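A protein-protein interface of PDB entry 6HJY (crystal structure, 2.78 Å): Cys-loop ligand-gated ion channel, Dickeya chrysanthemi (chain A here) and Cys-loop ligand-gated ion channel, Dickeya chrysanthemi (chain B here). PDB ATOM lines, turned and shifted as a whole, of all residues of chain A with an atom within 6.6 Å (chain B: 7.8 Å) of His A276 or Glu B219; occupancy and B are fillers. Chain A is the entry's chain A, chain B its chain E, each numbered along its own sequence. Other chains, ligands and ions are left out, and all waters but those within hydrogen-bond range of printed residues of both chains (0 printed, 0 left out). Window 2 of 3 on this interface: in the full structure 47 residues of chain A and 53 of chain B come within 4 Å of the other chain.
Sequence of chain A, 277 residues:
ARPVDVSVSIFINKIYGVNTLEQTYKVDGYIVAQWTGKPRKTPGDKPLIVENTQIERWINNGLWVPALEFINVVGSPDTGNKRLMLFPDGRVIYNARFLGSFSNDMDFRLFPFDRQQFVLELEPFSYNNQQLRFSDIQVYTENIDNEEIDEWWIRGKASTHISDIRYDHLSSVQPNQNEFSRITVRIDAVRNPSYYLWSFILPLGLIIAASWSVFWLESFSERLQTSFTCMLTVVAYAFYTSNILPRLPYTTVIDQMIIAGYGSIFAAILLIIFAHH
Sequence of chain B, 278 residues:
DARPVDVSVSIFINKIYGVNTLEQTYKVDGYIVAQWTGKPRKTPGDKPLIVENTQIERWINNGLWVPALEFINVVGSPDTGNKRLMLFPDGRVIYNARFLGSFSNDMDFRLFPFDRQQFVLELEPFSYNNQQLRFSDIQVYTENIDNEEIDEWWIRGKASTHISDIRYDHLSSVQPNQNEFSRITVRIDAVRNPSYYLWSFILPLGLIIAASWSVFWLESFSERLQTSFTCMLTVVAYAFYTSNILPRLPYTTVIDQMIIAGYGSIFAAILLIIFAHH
OE1 of Glu B223 sits at hydrogen-bond distance from OG of Ser A221 (3.0 Å).
The guanidinium group (NH2) of Arg B224 lies within hydrogen-bond range of the backbone carbonyl oxygen (O) of Glu B219, at 3.5 Å.
The side-chain carboxylate (OE2) of Glu B223 is in hydrogen-bond range of the side-chain hydroxyl (OG) of Ser B220 (2.8 Å).
Among the printed residues, pairs that only touch across the chains: His A277 with Trp B217 (3.4 Å), Phe A220 with Trp B217 (3.4 Å), His A276 with Glu B219 (3.4 Å) and His A277 with Glu B219 (3.6 Å).
Printed residues of chain B within 4 Å of Phe A220: Trp B217 (3.4 Å).
No residue of chain B comes within 4 Å of Ala A275.
Of chain B, only Glu B219 comes within 4 Å of His A276.
Of the printed residues of chain B, His A277 touches Trp B217 (3.4 Å) and Glu B219 (3.6 Å).
Of the printed residues of chain A, Trp B217 touches Phe A220 (3.4 Å) and His A277 (3.4 Å).
Glu B219 touches just these residues of chain A: His A276 (3.4 Å) and His A277 (3.6 Å).
Printed residues of chain A within 4 Å of Glu B223: Ser A221 (3.0 Å).
The nearest residue of chain B that does not touch His A276 is Trp B217 (4.9 Å).
The nearest residue of chain A that does not touch Glu B219 is Phe A220 (4.6 Å).
Hydrophobic or aromatic side chains of chain B within 4 Å of the printed part of chain A: Trp B217.
Along chain B the printed residues that touch a printed residue of chain A span positions 217 to 223.
Of the 10 printed residues of chain A, 4 touch a printed residue of chain B.
Among the printed residues, 5 pairs touch across the chains.
Among the printed residues, no Asp or Glu carboxylate lies within 4 Å of a Lys or Arg side-chain nitrogen of the other chain.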
ATOM      1  N   PHE A 220      16.223 -18.349   1.494  1.00  0.00           N
ATOM      2  CA  PHE A 220      16.872 -17.215   2.158  1.00  0.00           C
ATOM      3  C   PHE A 220      18.220 -17.644   2.750  1.00  0.00           C
ATOM      4  O   PHE A 220      19.173 -16.858   2.735  1.00  0.00           O
ATOM      5  CB  PHE A 220      15.942 -16.660   3.258  1.00  0.00           C
ATOM      6  CG  PHE A 220      16.538 -15.641   4.208  1.00  0.00           C
ATOM      7  CD1 PHE A 220      16.780 -14.338   3.793  1.00  0.00           C
ATOM      8  CD2 PHE A 220      16.812 -15.974   5.530  1.00  0.00           C
ATOM      9  CE1 PHE A 220      17.313 -13.390   4.675  1.00  0.00           C
ATOM     10  CE2 PHE A 220      17.347 -15.026   6.413  1.00  0.00           C
ATOM     11  CZ  PHE A 220      17.593 -13.743   5.978  1.00  0.00           C
ATOM     12  N   SER A 221      18.291 -18.899   3.253  1.00  0.00           N
ATOM     13  CA  SER A 221      19.482 -19.529   3.838  1.00  0.00           C
ATOM     14  C   SER A 221      20.596 -19.677   2.797  1.00  0.00           C
ATOM     15  O   SER A 221      21.768 -19.476   3.122  1.00  0.00           O
ATOM     16  CB  SER A 221      19.129 -20.891   4.425  1.00  0.00           C
ATOM     17  OG  SER A 221      20.230 -21.477   5.100  1.00  0.00           O
ATOM     18  N   ARG A 223      20.699 -17.842  -0.286  1.00  0.00           N
ATOM     19  CA  ARG A 223      20.963 -16.479  -0.781  1.00  0.00           C
ATOM     20  C   ARG A 223      21.949 -15.705   0.091  1.00  0.00           C
ATOM     21  O   ARG A 223      22.816 -15.010  -0.439  1.00  0.00           O
ATOM     22  CB  ARG A 223      19.659 -15.671  -0.916  1.00  0.00           C
ATOM     23  CG  ARG A 223      18.813 -16.060  -2.116  1.00  0.00           C
ATOM     24  CD  ARG A 223      17.711 -15.054  -2.396  1.00  0.00           C
ATOM     25  NE  ARG A 223      16.709 -15.010  -1.328  1.00  0.00           N
ATOM     26  CZ  ARG A 223      15.635 -15.793  -1.256  1.00  0.00           C
ATOM     27  NH1 ARG A 223      15.418 -16.721  -2.182  1.00  0.00           N
ATOM     28  NH2 ARG A 223      14.777 -15.662  -0.254  1.00  0.00           N
ATOM     29  N   LEU A 271      18.997  -6.042   0.036  1.00  0.00           N
ATOM     30  CA  LEU A 271      17.890  -6.453  -0.824  1.00  0.00           C
ATOM     31  C   LEU A 271      17.310  -7.806  -0.373  1.00  0.00           C
ATOM     32  O   LEU A 271      16.085  -7.962  -0.362  1.00  0.00           O
ATOM     33  CB  LEU A 271      18.363  -6.498  -2.295  1.00  0.00           C
ATOM     34  CG  LEU A 271      18.128  -5.246  -3.174  1.00  0.00           C
ATOM     35  CD1 LEU A 271      18.994  -4.051  -2.745  1.00  0.00           C
ATOM     36  CD2 LEU A 271      18.445  -5.545  -4.615  1.00  0.00           C
ATOM     37  N   ILE A 272      18.186  -8.763   0.027  1.00  0.00           N
ATOM     38  CA  ILE A 272      17.806 -10.094   0.522  1.00  0.00           C
ATOM     39  C   ILE A 272      17.006  -9.951   1.830  1.00  0.00           C
ATOM     40  O   ILE A 272      15.941 -10.557   1.952  1.00  0.00           O
ATOM     41  CB  ILE A 272      19.040 -11.048   0.650  1.00  0.00           C
ATOM     42  CG1 ILE A 272      19.657 -11.353  -0.731  1.00  0.00           C
ATOM     43  CG2 ILE A 272      18.682 -12.363   1.373  1.00  0.00           C
ATOM     44  CD1 ILE A 272      21.145 -11.735  -0.709  1.00  0.00           C
ATOM     45  N   ILE A 273      17.501  -9.116   2.774  1.00  0.00           N
ATOM     46  CA  ILE A 273      16.872  -8.823   4.074  1.00  0.00           C
ATOM     47  C   ILE A 273      15.499  -8.141   3.877  1.00  0.00           C
ATOM     48  O   ILE A 273      14.544  -8.472   4.587  1.00  0.00           O
ATOM     49  CB  ILE A 273      17.831  -8.011   5.013  1.00  0.00           C
ATOM     50  CG1 ILE A 273      19.150  -8.773   5.271  1.00  0.00           C
ATOM     51  CG2 ILE A 273      17.154  -7.634   6.356  1.00  0.00           C
ATOM     52  CD1 ILE A 273      20.352  -7.906   5.711  1.00  0.00           C
ATOM     53  N   PHE A 274      15.392  -7.246   2.871  1.00  0.00           N
ATOM     54  CA  PHE A 274      14.168  -6.509   2.533  1.00  0.00           C
ATOM     55  C   PHE A 274      13.096  -7.379   1.817  1.00  0.00           C
ATOM     56  O   PHE A 274      12.190  -6.849   1.168  1.00  0.00           O
ATOM     57  CB  PHE A 274      14.516  -5.241   1.725  1.00  0.00           C
ATOM     58  CG  PHE A 274      13.653  -4.034   2.021  1.00  0.00           C
ATOM     59  CD1 PHE A 274      13.954  -3.187   3.081  1.00  0.00           C
ATOM     60  CD2 PHE A 274      12.557  -3.730   1.225  1.00  0.00           C
ATOM     61  CE1 PHE A 274      13.155  -2.072   3.354  1.00  0.00           C
ATOM     62  CE2 PHE A 274      11.756  -2.617   1.500  1.00  0.00           C
ATOM     63  CZ  PHE A 274      12.063  -1.795   2.560  1.00  0.00           C
ATOM     64  N   ALA A 275      13.185  -8.708   1.967  1.00  0.00           N
ATOM     65  CA  ALA A 275      12.234  -9.651   1.384  1.00  0.00           C
ATOM     66  C   ALA A 275      11.727 -10.638   2.440  1.00  0.00           C
ATOM     67  O   ALA A 275      10.527 -10.906   2.493  1.00  0.00           O
ATOM     68  CB  ALA A 275      12.890 -10.403   0.235  1.00  0.00           C
ATOM     69  N   HIS A 276      12.638 -11.149   3.294  1.00  0.00           N
ATOM     70  CA  HIS A 276      12.332 -12.121   4.338  1.00  0.00           C
ATOM     71  C   HIS A 276      11.675 -11.476   5.562  1.00  0.00           C
ATOM     72  O   HIS A 276      10.479 -11.678   5.774  1.00  0.00           O
ATOM     73  CB  HIS A 276      13.597 -12.903   4.724  1.00  0.00           C
ATOM     74  CG  HIS A 276      13.336 -14.324   5.125  1.00  0.00           C
ATOM     75  ND1 HIS A 276      13.671 -14.793   6.381  1.00  0.00           N
ATOM     76  CD2 HIS A 276      12.796 -15.336   4.408  1.00  0.00           C
ATOM     77  CE1 HIS A 276      13.325 -16.068   6.390  1.00  0.00           C
ATOM     78  NE2 HIS A 276      12.793 -16.441   5.224  1.00  0.00           N
ATOM     79  N   HIS A 277      12.446 -10.698   6.355  1.00  0.00           N
ATOM     80  CA  HIS A 277      11.962 -10.018   7.558  1.00  0.00           C
ATOM     81  C   HIS A 277      11.525  -8.584   7.255  1.00  0.00           C
ATOM     82  O   HIS A 277      12.309  -7.786   6.745  1.00  0.00           O
ATOM     83  CB  HIS A 277      13.039 -10.032   8.657  1.00  0.00           C
ATOM     84  CG  HIS A 277      13.129 -11.325   9.413  1.00  0.00           C
ATOM     85  ND1 HIS A 277      13.936 -12.363   8.985  1.00  0.00           N
ATOM     86  CD2 HIS A 277      12.545 -11.679  10.582  1.00  0.00           C
ATOM     87  CE1 HIS A 277      13.802 -13.317   9.889  1.00  0.00           C
ATOM     88  NE2 HIS A 277      12.976 -12.954  10.869  1.00  0.00           N
ATOM     89  N   VAL B 215      23.721 -11.991  10.791  1.00  0.00           N
ATOM     90  CA  VAL B 215      23.654 -13.445  11.013  1.00  0.00           C
ATOM     91  C   VAL B 215      22.487 -13.827  11.938  1.00  0.00           C
ATOM     92  O   VAL B 215      21.911 -14.900  11.763  1.00  0.00           O
ATOM     93  CB  VAL B 215      24.997 -14.099  11.464  1.00  0.00           C
ATOM     94  CG1 VAL B 215      26.077 -13.944  10.398  1.00  0.00           C
ATOM     95  CG2 VAL B 215      25.480 -13.580  12.818  1.00  0.00           C
ATOM     96  N   PHE B 216      22.117 -12.926  12.877  1.00  0.00           N
ATOM     97  CA  PHE B 216      21.030 -13.086  13.849  1.00  0.00           C
ATOM     98  C   PHE B 216      19.655 -13.226  13.188  1.00  0.00           C
ATOM     99  O   PHE B 216      18.708 -13.701  13.822  1.00  0.00           O
ATOM    100  CB  PHE B 216      21.047 -11.932  14.868  1.00  0.00           C
ATOM    101  CG  PHE B 216      22.200 -12.001  15.838  1.00  0.00           C
ATOM    102  CD1 PHE B 216      22.066 -12.658  17.055  1.00  0.00           C
ATOM    103  CD2 PHE B 216      23.425 -11.428  15.528  1.00  0.00           C
ATOM    104  CE1 PHE B 216      23.139 -12.739  17.947  1.00  0.00           C
ATOM    105  CE2 PHE B 216      24.499 -11.510  16.420  1.00  0.00           C
ATOM    106  CZ  PHE B 216      24.348 -12.167  17.623  1.00  0.00           C
ATOM    107  N   TRP B 217      19.564 -12.846  11.900  1.00  0.00           N
ATOM    108  CA  TRP B 217      18.357 -12.923  11.082  1.00  0.00           C
ATOM    109  C   TRP B 217      18.175 -14.303  10.425  1.00  0.00           C
ATOM    110  O   TRP B 217      17.140 -14.542   9.798  1.00  0.00           O
ATOM    111  CB  TRP B 217      18.326 -11.779  10.057  1.00  0.00           C
ATOM    112  CG  TRP B 217      18.276 -10.423  10.701  1.00  0.00           C
ATOM    113  CD1 TRP B 217      19.333  -9.611  10.988  1.00  0.00           C
ATOM    114  CD2 TRP B 217      17.106  -9.747  11.186  1.00  0.00           C
ATOM    115  NE1 TRP B 217      18.893  -8.457  11.597  1.00  0.00           N
ATOM    116  CE2 TRP B 217      17.529  -8.515  11.733  1.00  0.00           C
ATOM    117  CE3 TRP B 217      15.737 -10.062  11.205  1.00  0.00           C
ATOM    118  CZ2 TRP B 217      16.629  -7.591  12.286  1.00  0.00           C
ATOM    119  CZ3 TRP B 217      14.846  -9.148  11.748  1.00  0.00           C
ATOM    120  CH2 TRP B 217      15.290  -7.929  12.281  1.00  0.00           C
ATOM    121  N   LEU B 218      19.160 -15.220  10.596  1.00  0.00           N
ATOM    122  CA  LEU B 218      19.084 -16.593  10.084  1.00  0.00           C
ATOM    123  C   LEU B 218      18.180 -17.422  11.000  1.00  0.00           C
ATOM    124  O   LEU B 218      18.181 -17.226  12.221  1.00  0.00           O
ATOM    125  CB  LEU B 218      20.471 -17.233   9.939  1.00  0.00           C
ATOM    126  CG  LEU B 218      21.294 -16.762   8.746  1.00  0.00           C
ATOM    127  CD1 LEU B 218      22.781 -16.796   9.066  1.00  0.00           C
ATOM    128  CD2 LEU B 218      20.986 -17.589   7.494  1.00  0.00           C
ATOM    129  N   GLU B 219      17.409 -18.339  10.401  1.00  0.00           N
ATOM    130  CA  GLU B 219      16.389 -19.149  11.063  1.00  0.00           C
ATOM    131  C   GLU B 219      16.898 -20.088  12.162  1.00  0.00           C
ATOM    132  O   GLU B 219      16.393 -20.035  13.284  1.00  0.00           O
ATOM    133  CB  GLU B 219      15.551 -19.933  10.027  1.00  0.00           C
ATOM    134  CG  GLU B 219      14.863 -19.069   8.974  1.00  0.00           C
ATOM    135  CD  GLU B 219      13.973 -17.965   9.517  1.00  0.00           C
ATOM    136  OE1 GLU B 219      12.823 -18.264   9.910  1.00  0.00           O
ATOM    137  OE2 GLU B 219      14.431 -16.799   9.566  1.00  0.00           O
ATOM    138  N   SER B 220      17.866 -20.938  11.851  1.00  0.00           N
ATOM    139  CA  SER B 220      18.372 -21.935  12.787  1.00  0.00           C
ATOM    140  C   SER B 220      19.745 -21.617  13.342  1.00  0.00           C
ATOM    141  O   SER B 220      20.481 -20.811  12.773  1.00  0.00           O
ATOM    142  CB  SER B 220      18.478 -23.258  12.059  1.00  0.00           C
ATOM    143  OG  SER B 220      19.465 -23.033  11.066  1.00  0.00           O
ATOM    144  N   PHE B 221      20.121 -22.359  14.396  1.00  0.00           N
ATOM    145  CA  PHE B 221      21.401 -22.303  15.094  1.00  0.00           C
ATOM    146  C   PHE B 221      22.543 -22.789  14.187  1.00  0.00           C
ATOM    147  O   PHE B 221      23.602 -22.166  14.177  1.00  0.00           O
ATOM    148  CB  PHE B 221      21.299 -23.148  16.379  1.00  0.00           C
ATOM    149  CG  PHE B 221      22.560 -23.379  17.180  1.00  0.00           C
ATOM    150  CD1 PHE B 221      23.034 -22.412  18.057  1.00  0.00           C
ATOM    151  CD2 PHE B 221      23.211 -24.606  17.141  1.00  0.00           C
ATOM    152  CE1 PHE B 221      24.174 -22.647  18.841  1.00  0.00           C
ATOM    153  CE2 PHE B 221      24.352 -24.840  17.921  1.00  0.00           C
ATOM    154  CZ  PHE B 221      24.813 -23.865  18.777  1.00  0.00           C
ATOM    155  N   SER B 222      22.314 -23.867  13.399  1.00  0.00           N
ATOM    156  CA  SER B 222      23.304 -24.441  12.468  1.00  0.00           C
ATOM    157  C   SER B 222      23.722 -23.442  11.379  1.00  0.00           C
ATOM    158  O   SER B 222      24.894 -23.406  10.997  1.00  0.00           O
ATOM    159  CB  SER B 222      22.768 -25.726  11.845  1.00  0.00           C
ATOM    160  OG  SER B 222      23.756 -26.414  11.095  1.00  0.00           O
ATOM    161  N   GLU B 223      22.767 -22.605  10.925  1.00  0.00           N
ATOM    162  CA  GLU B 223      22.979 -21.565   9.915  1.00  0.00           C
ATOM    163  C   GLU B 223      23.740 -20.369  10.501  1.00  0.00           C
ATOM    164  O   GLU B 223      24.706 -19.914   9.892  1.00  0.00           O
ATOM    165  CB  GLU B 223      21.637 -21.108   9.307  1.00  0.00           C
ATOM    166  CG  GLU B 223      21.005 -22.125   8.364  1.00  0.00           C
ATOM    167  CD  GLU B 223      19.507 -21.959   8.153  1.00  0.00           C
ATOM    168  OE1 GLU B 223      19.070 -20.844   7.789  1.00  0.00           O
ATOM    169  OE2 GLU B 223      18.768 -22.954   8.334  1.00  0.00           O
ATOM    170  N   ARG B 224      23.314 -19.881  11.691  1.00  0.00           N
ATOM    171  CA  ARG B 224      23.895 -18.734  12.407  1.00  0.00           C
ATOM    172  C   ARG B 224      25.374 -18.920  12.763  1.00  0.00           C
ATOM    173  O   ARG B 224      26.156 -17.978  12.626  1.00  0.00           O
ATOM    174  CB  ARG B 224      23.077 -18.392  13.668  1.00  0.00           C
ATOM    175  CG  ARG B 224      21.726 -17.772  13.348  1.00  0.00           C
ATOM    176  CD  ARG B 224      20.992 -17.323  14.598  1.00  0.00           C
ATOM    177  NE  ARG B 224      19.804 -18.147  14.839  1.00  0.00           N
ATOM    178  CZ  ARG B 224      19.699 -19.061  15.801  1.00  0.00           C
ATOM    179  NH1 ARG B 224      20.710 -19.284  16.631  1.00  0.00           N
ATOM    180  NH2 ARG B 224      18.574 -19.752  15.948  1.00  0.00           N
